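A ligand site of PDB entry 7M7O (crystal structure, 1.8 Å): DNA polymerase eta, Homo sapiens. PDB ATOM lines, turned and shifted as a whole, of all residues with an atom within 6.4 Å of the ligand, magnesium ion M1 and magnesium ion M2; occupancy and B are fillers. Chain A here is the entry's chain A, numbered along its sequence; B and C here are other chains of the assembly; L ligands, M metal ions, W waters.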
ATOM      1  N   ASP A  16      10.996   4.799 -29.688  1.00  0.00           N
ATOM      2  CA  ASP A  16      11.956   5.479 -28.817  1.00  0.00           C
ATOM      3  C   ASP A  16      12.311   6.845 -29.397  1.00  0.00           C
ATOM      4  O   ASP A  16      12.758   6.929 -30.542  1.00  0.00           O
ATOM      5  CB  ASP A  16      13.185   4.636 -28.631  1.00  0.00           C
ATOM      6  CG  ASP A  16      14.162   5.236 -27.655  1.00  0.00           C
ATOM      7  OD1 ASP A  16      14.847   6.178 -28.056  1.00  0.00           O
ATOM      8  OD2 ASP A  16      14.162   4.814 -26.480  1.00  0.00           O
ATOM      9  N   MET A  17      12.155   7.896 -28.585  1.00  0.00           N
ATOM     10  CA  MET A  17      12.366   9.241 -29.097  1.00  0.00           C
ATOM     11  C   MET A  17      13.848   9.445 -29.432  1.00  0.00           C
ATOM     12  O   MET A  17      14.731   8.922 -28.747  1.00  0.00           O
ATOM     13  CB  MET A  17      11.940  10.279 -28.062  1.00  0.00           C
ATOM     14  CG  MET A  17      10.508  10.102 -27.552  1.00  0.00           C
ATOM     15  SD  MET A  17       9.305   9.994 -28.927  1.00  0.00           S
ATOM     16  CE  MET A  17       9.479  11.583 -29.665  1.00  0.00           C
ATOM     17  N   ASP A  18      14.119  10.187 -30.497  1.00  0.00           N
ATOM     18  CA  ASP A  18      15.512  10.474 -30.845  1.00  0.00           C
ATOM     19  C   ASP A  18      16.030  11.603 -29.953  1.00  0.00           C
ATOM     20  O   ASP A  18      15.315  12.583 -29.720  1.00  0.00           O
ATOM     21  CB  ASP A  18      15.601  10.893 -32.299  1.00  0.00           C
ATOM     22  CG  ASP A  18      15.172   9.778 -33.263  1.00  0.00           C
ATOM     23  OD1 ASP A  18      15.312   8.585 -32.914  1.00  0.00           O
ATOM     24  OD2 ASP A  18      14.751  10.092 -34.391  1.00  0.00           O
ATOM     25  N   CYS A  19      17.244  11.420 -29.396  1.00  0.00           N
ATOM     26  CA  CYS A  19      17.870  12.388 -28.496  1.00  0.00           C
ATOM     27  C   CYS A  19      16.855  13.245 -27.721  1.00  0.00           C
ATOM     28  O   CYS A  19      16.822  14.476 -27.883  1.00  0.00           O
ATOM     29  CB  CYS A  19      18.813  13.300 -29.283  1.00  0.00           C
ATOM     30  SG  CYS A  19      18.036  14.145 -30.685  1.00  0.00           S
ATOM     31  N   PHE A  20      16.031  12.598 -26.904  1.00  0.00           N
ATOM     32  CA  PHE A  20      14.751  13.142 -26.451  1.00  0.00           C
ATOM     33  C   PHE A  20      14.918  14.498 -25.742  1.00  0.00           C
ATOM     34  O   PHE A  20      14.230  15.466 -26.080  1.00  0.00           O
ATOM     35  CB  PHE A  20      14.006  12.161 -25.558  1.00  0.00           C
ATOM     36  CG  PHE A  20      12.649  12.631 -25.133  1.00  0.00           C
ATOM     37  CD1 PHE A  20      11.777  13.160 -26.079  1.00  0.00           C
ATOM     38  CD2 PHE A  20      12.228  12.534 -23.806  1.00  0.00           C
ATOM     39  CE1 PHE A  20      10.488  13.582 -25.718  1.00  0.00           C
ATOM     40  CE2 PHE A  20      10.942  12.975 -23.432  1.00  0.00           C
ATOM     41  CZ  PHE A  20      10.074  13.494 -24.398  1.00  0.00           C
ATOM     42  N   PHE A  21      15.742  14.568 -24.680  1.00  0.00           N
ATOM     43  CA  PHE A  21      15.765  15.843 -23.951  1.00  0.00           C
ATOM     44  C   PHE A  21      16.266  16.968 -24.850  1.00  0.00           C
ATOM     45  O   PHE A  21      15.823  18.115 -24.728  1.00  0.00           O
ATOM     46  CB  PHE A  21      16.634  15.786 -22.691  1.00  0.00           C
ATOM     47  CG  PHE A  21      16.106  14.917 -21.580  1.00  0.00           C
ATOM     48  CD1 PHE A  21      15.025  14.047 -21.762  1.00  0.00           C
ATOM     49  CD2 PHE A  21      16.667  15.023 -20.317  1.00  0.00           C
ATOM     50  CE1 PHE A  21      14.552  13.261 -20.707  1.00  0.00           C
ATOM     51  CE2 PHE A  21      16.194  14.264 -19.255  1.00  0.00           C
ATOM     52  CZ  PHE A  21      15.141  13.370 -19.455  1.00  0.00           C
ATOM     53  N   VAL A  22      17.176  16.647 -25.770  1.00  0.00           N
ATOM     54  CA  VAL A  22      17.646  17.630 -26.740  1.00  0.00           C
ATOM     55  C   VAL A  22      16.496  18.112 -27.611  1.00  0.00           C
ATOM     56  O   VAL A  22      16.344  19.316 -27.843  1.00  0.00           O
ATOM     57  CB  VAL A  22      18.792  17.054 -27.595  1.00  0.00           C
ATOM     58  CG1 VAL A  22      19.058  17.957 -28.796  1.00  0.00           C
ATOM     59  CG2 VAL A  22      20.031  16.932 -26.719  1.00  0.00           C
ATOM     60  N   GLN A  41      23.308  18.820 -16.838  1.00  0.00           N
ATOM     61  CA  GLN A  41      22.777  19.110 -15.513  1.00  0.00           C
ATOM     62  C   GLN A  41      23.906  19.570 -14.603  1.00  0.00           C
ATOM     63  O   GLN A  41      24.981  18.975 -14.611  1.00  0.00           O
ATOM     64  CB  GLN A  41      22.010  17.916 -14.919  1.00  0.00           C
ATOM     65  CG  GLN A  41      22.602  16.576 -15.049  1.00  0.00           C
ATOM     66  CD  GLN A  41      21.674  15.516 -14.441  1.00  0.00           C
ATOM     67  OE1 GLN A  41      20.436  15.676 -14.405  1.00  0.00           O
ATOM     68  NE2 GLN A  41      22.264  14.439 -14.029  1.00  0.00           N
ATOM     69  N   ILE A  51      23.626  14.704 -20.333  1.00  0.00           N
ATOM     70  CA  ILE A  51      22.684  13.595 -20.274  1.00  0.00           C
ATOM     71  C   ILE A  51      21.975  13.310 -21.587  1.00  0.00           C
ATOM     72  O   ILE A  51      21.304  12.267 -21.674  1.00  0.00           O
ATOM     73  CB  ILE A  51      21.639  13.779 -19.155  1.00  0.00           C
ATOM     74  CG1 ILE A  51      20.830  15.055 -19.371  1.00  0.00           C
ATOM     75  CG2 ILE A  51      22.341  13.727 -17.764  1.00  0.00           C
ATOM     76  CD1 ILE A  51      19.724  15.191 -18.375  1.00  0.00           C
ATOM     77  N   ALA A  52      22.129  14.151 -22.618  1.00  0.00           N
ATOM     78  CA  ALA A  52      21.528  13.880 -23.924  1.00  0.00           C
ATOM     79  C   ALA A  52      22.312  14.658 -24.981  1.00  0.00           C
ATOM     80  O   ALA A  52      22.766  15.777 -24.732  1.00  0.00           O
ATOM     81  CB  ALA A  52      20.047  14.292 -23.912  1.00  0.00           C
ATOM     82  N   VAL A  53      22.424  14.082 -26.198  1.00  0.00           N
ATOM     83  CA  VAL A  53      23.354  14.591 -27.204  1.00  0.00           C
ATOM     84  C   VAL A  53      22.674  14.534 -28.571  1.00  0.00           C
ATOM     85  O   VAL A  53      22.206  13.460 -28.990  1.00  0.00           O
ATOM     86  CB  VAL A  53      24.661  13.759 -27.242  1.00  0.00           C
ATOM     87  CG1 VAL A  53      25.668  14.403 -28.173  1.00  0.00           C
ATOM     88  CG2 VAL A  53      25.216  13.526 -25.840  1.00  0.00           C
ATOM     89  N   TYR A  55      22.368  14.337 -32.659  1.00  0.00           N
ATOM     90  CA  TYR A  55      23.143  13.502 -33.583  1.00  0.00           C
ATOM     91  C   TYR A  55      24.281  14.291 -34.229  1.00  0.00           C
ATOM     92  O   TYR A  55      25.393  13.757 -34.408  1.00  0.00           O
ATOM     93  CB  TYR A  55      22.224  12.853 -34.595  1.00  0.00           C
ATOM     94  CG  TYR A  55      21.538  11.677 -33.950  1.00  0.00           C
ATOM     95  CD1 TYR A  55      20.429  11.851 -33.123  1.00  0.00           C
ATOM     96  CD2 TYR A  55      22.025  10.402 -34.139  1.00  0.00           C
ATOM     97  CE1 TYR A  55      19.825  10.746 -32.523  1.00  0.00           C
ATOM     98  CE2 TYR A  55      21.450   9.307 -33.517  1.00  0.00           C
ATOM     99  CZ  TYR A  55      20.353   9.468 -32.721  1.00  0.00           C
ATOM    100  OH  TYR A  55      19.761   8.356 -32.120  1.00  0.00           O
ATOM    101  N   ARG A  58      26.978  14.072 -31.672  1.00  0.00           N
ATOM    102  CA  ARG A  58      27.556  12.730 -31.577  1.00  0.00           C
ATOM    103  C   ARG A  58      28.613  12.504 -32.649  1.00  0.00           C
ATOM    104  O   ARG A  58      29.582  11.746 -32.415  1.00  0.00           O
ATOM    105  CB  ARG A  58      26.489  11.647 -31.704  1.00  0.00           C
ATOM    106  CG  ARG A  58      25.446  11.729 -30.669  1.00  0.00           C
ATOM    107  CD  ARG A  58      24.440  10.622 -30.811  1.00  0.00           C
ATOM    108  NE  ARG A  58      23.263  10.953 -30.001  1.00  0.00           N
ATOM    109  CZ  ARG A  58      22.273  10.121 -29.723  1.00  0.00           C
ATOM    110  NH1 ARG A  58      22.311   8.864 -30.166  1.00  0.00           N
ATOM    111  NH2 ARG A  58      21.242  10.546 -28.954  1.00  0.00           N
ATOM    112  N   ARG A  64      26.742  10.938 -23.780  1.00  0.00           N
ATOM    113  CA  ARG A  64      26.207  10.904 -22.422  1.00  0.00           C
ATOM    114  C   ARG A  64      27.305  10.602 -21.404  1.00  0.00           C
ATOM    115  O   ARG A  64      28.267   9.864 -21.703  1.00  0.00           O
ATOM    116  CB  ARG A  64      25.092   9.854 -22.348  1.00  0.00           C
ATOM    117  CG  ARG A  64      24.237   9.815 -21.075  1.00  0.00           C
ATOM    118  CD  ARG A  64      23.017   8.917 -21.296  1.00  0.00           C
ATOM    119  NE  ARG A  64      23.420   7.690 -21.987  1.00  0.00           N
ATOM    120  CZ  ARG A  64      22.633   6.962 -22.783  1.00  0.00           C
ATOM    121  NH1 ARG A  64      21.372   7.304 -23.011  1.00  0.00           N
ATOM    122  NH2 ARG A  64      23.125   5.868 -23.364  1.00  0.00           N
ATOM    123  N   LEU A  92      13.192  17.470 -13.499  1.00  0.00           N
ATOM    124  CA  LEU A  92      12.961  16.918 -14.824  1.00  0.00           C
ATOM    125  C   LEU A  92      11.538  17.106 -15.334  1.00  0.00           C
ATOM    126  O   LEU A  92      11.143  16.472 -16.317  1.00  0.00           O
ATOM    127  CB  LEU A  92      13.339  15.436 -14.851  1.00  0.00           C
ATOM    128  CG  LEU A  92      14.802  15.251 -14.403  1.00  0.00           C
ATOM    129  CD1 LEU A  92      15.151  13.758 -14.281  1.00  0.00           C
ATOM    130  CD2 LEU A  92      15.748  16.041 -15.310  1.00  0.00           C
ATOM    131  N   SER A 116      10.196   3.746 -20.485  1.00  0.00           N
ATOM    132  CA  SER A 116      11.058   4.778 -19.913  1.00  0.00           C
ATOM    133  C   SER A 116      10.439   6.135 -20.199  1.00  0.00           C
ATOM    134  O   SER A 116       9.343   6.238 -20.753  1.00  0.00           O
ATOM    135  CB  SER A 116      12.450   4.622 -20.519  1.00  0.00           C
ATOM    136  OG  SER A 116      12.510   5.293 -21.770  1.00  0.00           O
ATOM    137  N   ILE A 117      11.107   7.200 -19.736  1.00  0.00           N
ATOM    138  CA  ILE A 117      10.597   8.525 -20.059  1.00  0.00           C
ATOM    139  C   ILE A 117      10.465   8.756 -21.561  1.00  0.00           C
ATOM    140  O   ILE A 117       9.629   9.579 -21.996  1.00  0.00           O
ATOM    141  CB  ILE A 117      11.471   9.616 -19.406  1.00  0.00           C
ATOM    142  CG1 ILE A 117      10.668  10.925 -19.364  1.00  0.00           C
ATOM    143  CG2 ILE A 117      12.712   9.829 -20.246  1.00  0.00           C
ATOM    144  CD1 ILE A 117      11.311  12.004 -18.441  1.00  0.00           C
ATOM    145  N   ASP A 118      11.233   8.040 -22.411  1.00  0.00           N
ATOM    146  CA  ASP A 118      11.183   8.375 -23.832  1.00  0.00           C
ATOM    147  C   ASP A 118      10.827   7.173 -24.715  1.00  0.00           C
ATOM    148  O   ASP A 118      10.989   7.244 -25.938  1.00  0.00           O
ATOM    149  CB  ASP A 118      12.526   8.980 -24.303  1.00  0.00           C
ATOM    150  CG  ASP A 118      13.491   7.948 -24.893  1.00  0.00           C
ATOM    151  OD1 ASP A 118      13.971   8.222 -26.033  1.00  0.00           O
ATOM    152  OD2 ASP A 118      13.766   6.864 -24.287  1.00  0.00           O
ATOM    153  N   GLU A 119      10.284   6.080 -24.152  1.00  0.00           N
ATOM    154  CA  GLU A 119       9.991   4.953 -25.040  1.00  0.00           C
ATOM    155  C   GLU A 119       8.865   4.104 -24.469  1.00  0.00           C
ATOM    156  O   GLU A 119       8.702   3.979 -23.237  1.00  0.00           O
ATOM    157  CB  GLU A 119      11.187   4.071 -25.306  1.00  0.00           C
ATOM    158  CG  GLU A 119      11.582   3.202 -24.165  1.00  0.00           C
ATOM    159  CD  GLU A 119      13.067   2.985 -24.190  1.00  0.00           C
ATOM    160  OE1 GLU A 119      13.487   1.871 -24.567  1.00  0.00           O
ATOM    161  OE2 GLU A 119      13.791   3.936 -23.843  1.00  0.00           O
ATOM    162  N   SER A 216      12.356   6.898 -33.441  1.00  0.00           N
ATOM    163  CA  SER A 216      12.665   5.697 -34.205  1.00  0.00           C
ATOM    164  C   SER A 216      11.811   4.572 -33.652  1.00  0.00           C
ATOM    165  O   SER A 216      11.207   4.694 -32.577  1.00  0.00           O
ATOM    166  CB  SER A 216      14.143   5.339 -34.092  1.00  0.00           C
ATOM    167  OG  SER A 216      14.927   6.386 -34.685  1.00  0.00           O
ATOM    168  N   LYS A 227      12.902  -3.894 -29.464  1.00  0.00           N
ATOM    169  CA  LYS A 227      13.892  -2.968 -28.901  1.00  0.00           C
ATOM    170  C   LYS A 227      15.207  -3.018 -29.684  1.00  0.00           C
ATOM    171  O   LYS A 227      15.821  -1.974 -29.982  1.00  0.00           O
ATOM    172  CB  LYS A 227      14.121  -3.272 -27.418  1.00  0.00           C
ATOM    173  CG  LYS A 227      15.282  -2.433 -26.766  1.00  0.00           C
ATOM    174  CD  LYS A 227      15.038  -0.925 -26.746  1.00  0.00           C
ATOM    175  CE  LYS A 227      16.084  -0.127 -25.925  1.00  0.00           C
ATOM    176  NZ  LYS A 227      15.853   1.393 -25.979  1.00  0.00           N
ATOM    177  N   LYS A 234      18.402   4.228 -36.155  1.00  0.00           N
ATOM    178  CA  LYS A 234      18.292   5.574 -35.588  1.00  0.00           C
ATOM    179  C   LYS A 234      19.243   6.554 -36.274  1.00  0.00           C
ATOM    180  O   LYS A 234      20.363   6.181 -36.641  1.00  0.00           O
ATOM    181  CB  LYS A 234      18.639   5.489 -34.095  1.00  0.00           C
ATOM    182  CG  LYS A 234      17.442   5.478 -33.187  1.00  0.00           C
ATOM    183  CD  LYS A 234      17.737   5.418 -31.681  1.00  0.00           C
ATOM    184  CE  LYS A 234      16.410   5.395 -30.897  1.00  0.00           C
ATOM    185  NZ  LYS A 234      15.801   6.792 -30.738  1.00  0.00           N
ATOM    186  N   PRO A 235      18.851   7.837 -36.435  1.00  0.00           N
ATOM    187  CA  PRO A 235      17.582   8.415 -35.970  1.00  0.00           C
ATOM    188  C   PRO A 235      16.530   8.508 -37.077  1.00  0.00           C
ATOM    189  O   PRO A 235      16.844   8.343 -38.282  1.00  0.00           O
ATOM    190  CB  PRO A 235      17.981   9.836 -35.541  1.00  0.00           C
ATOM    191  CG  PRO A 235      19.052  10.192 -36.565  1.00  0.00           C
ATOM    192  CD  PRO A 235      19.777   8.889 -36.903  1.00  0.00           C
ATOM    193  P    DT B   9      18.797   0.462 -22.078  1.00  0.00           P
ATOM    194  OP1  DT B   9      18.369   0.202 -23.466  1.00  0.00           O
ATOM    195  OP2  DT B   9      20.216   0.632 -21.754  1.00  0.00           O
ATOM    196  O5'  DT B   9      18.138   1.795 -21.523  1.00  0.00           O
ATOM    197  C5'  DT B   9      16.692   2.174 -21.659  1.00  0.00           C
ATOM    198  C4'  DT B   9      16.045   3.502 -21.275  1.00  0.00           C
ATOM    199  O4'  DT B   9      16.414   3.772 -19.900  1.00  0.00           O
ATOM    200  C3'  DT B   9      16.659   4.631 -22.100  1.00  0.00           C
ATOM    201  O3'  DT B   9      15.710   5.559 -22.604  1.00  0.00           O
ATOM    202  C2'  DT B   9      17.741   5.203 -21.197  1.00  0.00           C
ATOM    203  C1'  DT B   9      17.171   4.966 -19.824  1.00  0.00           C
ATOM    204  N1   DT B   9      18.198   4.795 -18.782  1.00  0.00           N
ATOM    205  C2   DT B   9      18.157   5.641 -17.693  1.00  0.00           C
ATOM    206  O2   DT B   9      17.306   6.497 -17.549  1.00  0.00           O
ATOM    207  N3   DT B   9      19.156   5.435 -16.767  1.00  0.00           N
ATOM    208  C4   DT B   9      20.164   4.495 -16.832  1.00  0.00           C
ATOM    209  O4   DT B   9      20.987   4.432 -15.931  1.00  0.00           O
ATOM    210  C5   DT B   9      20.154   3.648 -18.002  1.00  0.00           C
ATOM    211  C7   DT B   9      21.210   2.598 -18.147  1.00  0.00           C
ATOM    212  C6   DT B   9      19.186   3.841 -18.905  1.00  0.00           C
ATOM    213  P    DT C   3      33.118  10.500 -12.054  1.00  0.00           P
ATOM    214  OP1  DT C   3      33.549   9.363 -11.219  1.00  0.00           O
ATOM    215  OP2  DT C   3      33.972  11.051 -13.137  1.00  0.00           O
ATOM    216  O5'  DT C   3      31.720  10.099 -12.715  1.00  0.00           O
ATOM    217  C5'  DT C   3      31.241  10.836 -13.834  1.00  0.00           C
ATOM    218  C4'  DT C   3      29.761  11.068 -13.674  1.00  0.00           C
ATOM    219  O4'  DT C   3      29.057  10.409 -14.744  1.00  0.00           O
ATOM    220  C3'  DT C   3      29.176  10.510 -12.388  1.00  0.00           C
ATOM    221  O3'  DT C   3      28.061  11.258 -12.002  1.00  0.00           O
ATOM    222  C2'  DT C   3      28.789   9.100 -12.780  1.00  0.00           C
ATOM    223  C1'  DT C   3      28.403   9.249 -14.241  1.00  0.00           C
ATOM    224  N1   DT C   3      28.816   8.100 -15.056  1.00  0.00           N
ATOM    225  C2   DT C   3      27.998   7.646 -16.050  1.00  0.00           C
ATOM    226  O2   DT C   3      26.916   8.163 -16.319  1.00  0.00           O
ATOM    227  N3   DT C   3      28.478   6.569 -16.748  1.00  0.00           N
ATOM    228  C4   DT C   3      29.685   5.908 -16.535  1.00  0.00           C
ATOM    229  O4   DT C   3      30.031   4.954 -17.209  1.00  0.00           O
ATOM    230  C5   DT C   3      30.501   6.437 -15.466  1.00  0.00           C
ATOM    231  C7   DT C   3      31.829   5.815 -15.144  1.00  0.00           C
ATOM    232  C6   DT C   3      30.028   7.497 -14.784  1.00  0.00           C
ATOM    233  P    DT C   4      27.578  11.237 -10.472  1.00  0.00           P
ATOM    234  OP1  DT C   4      28.425  12.131  -9.664  1.00  0.00           O
ATOM    235  OP2  DT C   4      27.312   9.814 -10.163  1.00  0.00           O
ATOM    236  O5'  DT C   4      26.162  11.948 -10.509  1.00  0.00           O
ATOM    237  C5'  DT C   4      26.043  13.246 -11.027  1.00  0.00           C
ATOM    238  C4'  DT C   4      24.588  13.518 -11.337  1.00  0.00           C
ATOM    239  O4'  DT C   4      24.207  12.723 -12.478  1.00  0.00           O
ATOM    240  C3'  DT C   4      23.617  13.120 -10.230  1.00  0.00           C
ATOM    241  O3'  DT C   4      22.596  14.062 -10.199  1.00  0.00           O
ATOM    242  C2'  DT C   4      23.111  11.738 -10.677  1.00  0.00           C
ATOM    243  C1'  DT C   4      23.060  11.939 -12.172  1.00  0.00           C
ATOM    244  N1   DT C   4      23.138  10.705 -12.994  1.00  0.00           N
ATOM    245  C2   DT C   4      22.326  10.609 -14.090  1.00  0.00           C
ATOM    246  O2   DT C   4      21.520  11.485 -14.398  1.00  0.00           O
ATOM    247  N3   DT C   4      22.485   9.479 -14.831  1.00  0.00           N
ATOM    248  C4   DT C   4      23.359   8.447 -14.592  1.00  0.00           C
ATOM    249  O4   DT C   4      23.407   7.460 -15.328  1.00  0.00           O
ATOM    250  C5   DT C   4      24.193   8.603 -13.417  1.00  0.00           C
ATOM    251  C7   DT C   4      25.185   7.536 -13.046  1.00  0.00           C
ATOM    252  C6   DT C   4      24.050   9.716 -12.696  1.00  0.00           C
ATOM    253  P    DA C   5      21.439  14.062  -9.006  1.00  0.00           P
ATOM    254  OP1  DA C   5      21.327  15.438  -8.494  1.00  0.00           O
ATOM    255  OP2  DA C   5      21.688  12.961  -8.041  1.00  0.00           O
ATOM    256  O5'  DA C   5      20.108  13.622  -9.759  1.00  0.00           O
ATOM    257  C5'  DA C   5      19.675  14.183 -11.013  1.00  0.00           C
ATOM    258  C4'  DA C   5      18.396  13.529 -11.491  1.00  0.00           C
ATOM    259  O4'  DA C   5      18.723  12.365 -12.283  1.00  0.00           O
ATOM    260  C3'  DA C   5      17.433  13.059 -10.414  1.00  0.00           C
ATOM    261  O3'  DA C   5      16.093  13.370 -10.807  1.00  0.00           O
ATOM    262  C2'  DA C   5      17.711  11.569 -10.309  1.00  0.00           C
ATOM    263  C1'  DA C   5      18.069  11.225 -11.744  1.00  0.00           C
ATOM    264  N9   DA C   5      18.971  10.087 -11.897  1.00  0.00           N
ATOM    265  C8   DA C   5      20.043   9.737 -11.109  1.00  0.00           C
ATOM    266  N7   DA C   5      20.669   8.666 -11.526  1.00  0.00           N
ATOM    267  C5   DA C   5      19.974   8.282 -12.660  1.00  0.00           C
ATOM    268  C6   DA C   5      20.140   7.219 -13.566  1.00  0.00           C
ATOM    269  N6   DA C   5      21.102   6.297 -13.458  1.00  0.00           N
ATOM    270  N1   DA C   5      19.265   7.126 -14.597  1.00  0.00           N
ATOM    271  C2   DA C   5      18.305   8.039 -14.700  1.00  0.00           C
ATOM    272  N3   DA C   5      18.043   9.090 -13.916  1.00  0.00           N
ATOM    273  C4   DA C   5      18.924   9.151 -12.903  1.00  0.00           C
HETATM  274  N1  LIG L   1      20.888   9.295 -16.891  1.00  0.00           N
HETATM  275  C1  LIG L   1      20.036  10.312 -17.018  1.00  0.00           C
HETATM  276  N2  LIG L   1      19.192  10.586 -17.996  1.00  0.00           N
HETATM  277  C2  LIG L   1      19.294   9.665 -18.971  1.00  0.00           C
HETATM  278  C3  LIG L   1      20.130   8.573 -18.999  1.00  0.00           C
HETATM  279  C4  LIG L   1      20.979   8.395 -17.889  1.00  0.00           C
HETATM  280  N3  LIG L   1      21.814   7.370 -17.812  1.00  0.00           N
HETATM  281  N4  LIG L   1      19.953   7.862 -20.169  1.00  0.00           N
HETATM  282  C5  LIG L   1      19.026   8.535 -20.811  1.00  0.00           C
HETATM  283  N5  LIG L   1      18.589   9.640 -20.131  1.00  0.00           N
HETATM  284  P1  LIG L   1      17.700   7.400 -24.559  1.00  0.00           P
HETATM  285  P2  LIG L   1      18.098   9.583 -26.390  1.00  0.00           P
HETATM  286  P3  LIG L   1      18.533   8.179 -28.851  1.00  0.00           P
HETATM  287  C6  LIG L   1      17.579  10.595 -20.501  1.00  0.00           C
HETATM  288  O1  LIG L   1      16.553   6.885 -25.272  1.00  0.00           O
HETATM  289  O2  LIG L   1      16.654   9.642 -26.534  1.00  0.00           O
HETATM  290  O3  LIG L   1      17.456   7.360 -28.253  1.00  0.00           O
HETATM  291  C7  LIG L   1      18.024  11.669 -21.484  1.00  0.00           C
HETATM  292  O4  LIG L   1      18.595   6.248 -24.070  1.00  0.00           O
HETATM  293  O5  LIG L   1      18.654  10.934 -25.878  1.00  0.00           O
HETATM  294  O6  LIG L   1      18.129   8.838 -30.115  1.00  0.00           O
HETATM  295  C8  LIG L   1      17.585  11.103 -22.824  1.00  0.00           C
HETATM  296  O7  LIG L   1      17.276  12.112 -23.774  1.00  0.00           O
HETATM  297  N6  LIG L   1      18.615   8.352 -25.496  1.00  0.00           N
HETATM  298  O8  LIG L   1      18.789   9.325 -27.794  1.00  0.00           O
HETATM  299  O9  LIG L   1      19.825   7.445 -28.983  1.00  0.00           O
HETATM  300  C9  LIG L   1      16.331  10.316 -22.460  1.00  0.00           C
HETATM  301  O10 LIG L   1      16.499   9.882 -21.097  1.00  0.00           O
HETATM  302  C10 LIG L   1      16.100   9.104 -23.325  1.00  0.00           C
HETATM  303  O11 LIG L   1      17.249   8.231 -23.279  1.00  0.00           O
HETATM  304 MG    MG M   1      15.721   7.883 -27.239  1.00  0.00          MG
HETATM  305 MG    MG M   2      15.033   5.412 -24.717  1.00  0.00          MG
HETATM  306  O   HOH W   1      15.006   7.297 -20.793  1.00  0.00           O
HETATM  307  O   HOH W   2      19.993   4.050 -24.146  1.00  0.00           O
HETATM  308  O   HOH W   3      16.641   4.131 -25.270  1.00  0.00           O
HETATM  309  O   HOH W   4      17.805   4.719 -27.682  1.00  0.00           O
HETATM  310  O   HOH W   5      21.557   7.221 -26.951  1.00  0.00           O
HETATM  311  O   HOH W   6      22.165   5.300 -20.016  1.00  0.00           O
HETATM  312  O   HOH W   7      20.778   9.680 -23.429  1.00  0.00           O
HETATM  313  O   HOH W   8      15.831   8.750 -17.922  1.00  0.00           O
HETATM  314  O   HOH W   9      21.212  11.533 -26.280  1.00  0.00           O
HETATM  315  O   HOH W  10      17.330  12.342 -16.729  1.00  0.00           O
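NZ of Lys 234 lies within salt-bridge range of O6 of the ligand. NH1 of Arg 58 is in salt-bridge range of O9 of the ligand (3.1 Å). The side-chain hydroxyl (OH) of Tyr 55 lies within hydrogen-bond range of an oxygen (O6) of the ligand. The backbone NH (N) of Cys 19 lies within hydrogen-bond range of an oxygen (O6) of the ligand (2.8 Å). A nitrogen (N3) of the ligand sits at hydrogen-bond distance from O4 of DT 4 of chain C, 3.0 Å away. N3 of DT 9 of chain B is in hydrogen-bond range of N3 of the ligand (3.4 Å). An oxygen (O7) of the ligand lies within hydrogen-bond range of the backbone NH (N) of Phe 21, 3.0 Å away. The guanidinium group (NH1) of Arg 64 is in salt-bridge range of an oxygen (O4) of the ligand, at 3.2 Å. An oxygen (O5) of the ligand sits at hydrogen-bond distance from the backbone NH (N) of Phe 20, 3.3 Å away.
NZ of Lys 234 lies within hydrogen-bond range of O of Asp 16, 3.1 Å away. The backbone NH of Asp 118 sits close to the side-chain hydroxyl of Ser 116, at 3.1 Å. NE of Arg 58 is in hydrogen-bond range of O of Val 53 (2.9 Å). The side-chain carboxylate (OE1) of Glu 119 is in salt-bridge range of the side-chain amino group (NZ) of Lys 227, 2.8 Å away. OP1 of DT 9 of chain B lies within salt-bridge range of the side-chain amino group of Lys 227 (3.8 Å). O of Met 17 lies close to NZ of Lys 234 (3.1 Å). OH of Tyr 55 sits at hydrogen-bond distance from NH1 of Arg 58. O3' of DT 9 of chain B lies close to OG of Ser 116 (3.3 Å).
Merely in contact with the ligand: Asp 18, Ile 51, Ala 52, DA 5 of chain C and Ile 117. Hydrophobic or aromatic side chains within 4 Å of the ligand: Phe 20, Phe 21, Ala 52, Tyr 55 and Ile 117. 17 residues have an atom within 4 Å of the ligand: Asp 16, Met 17, Asp 18, Cys 19, Phe 20, Phe 21, Ile 51, Ala 52, Tyr 55, Arg 58, Arg 64, Ile 117, Asp 118, Lys 234, DT 9 of chain B, DT 4 of chain C and DA 5 of chain C. The nearest printed residue that does not touch the ligand is Glu 119 (4.3 Å).
NZ of Lys 234 touches magnesium ion M1 (3.7 Å).
Merely in contact with magnesium ion M2: Ser 116. Along chain A the residues within 4 Å of magnesium ion M2 span positions 16 to 119.
Magnesium ion M1 is bound by O3 of the ligand (2.1 Å), O of Met 17 (2.1 Å), OD1 of Asp 16 (2.1 Å), O2 of the ligand (2.1 Å), OD1 of Asp 118 (2.2 Å) and O1 of the ligand (2.4 Å).
Magnesium ion M2 is bound by OD2 of Asp 118 (2.0 Å), OD2 of Asp 16 (2.1 Å), OE2 of Glu 119 (2.1 Å), water W3 (2.1 Å), O1 of the ligand (2.2 Å) and O3' of DT 9 of chain B (2.2 Å).
Water W3 bridges NZ of Lys 227 (2.9 Å) and O4 of the ligand (3.1 Å). Water W9 lies within hydrogen-bond range of O5 of the ligand, N of Val 53 and NH2 of Arg 58. Water W1 bridges O10 of the ligand (3.0 Å) and OG of Ser 116 (3.3 Å). Water W6 lies within hydrogen-bond range of a nitrogen (N3) of the ligand (3.0 Å) and the guanidinium group (NE) of Arg 64 (3.3 Å). Water W7 lies within hydrogen-bond range of NH1 of Arg 64 (2.5 Å), O of Ile 51 (3.2 Å) and N6 of the ligand (3.3 Å). Water W8 bridges O2 of DT 9 of chain B (2.7 Å) and an oxygen (O10) of the ligand (3.4 Å).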
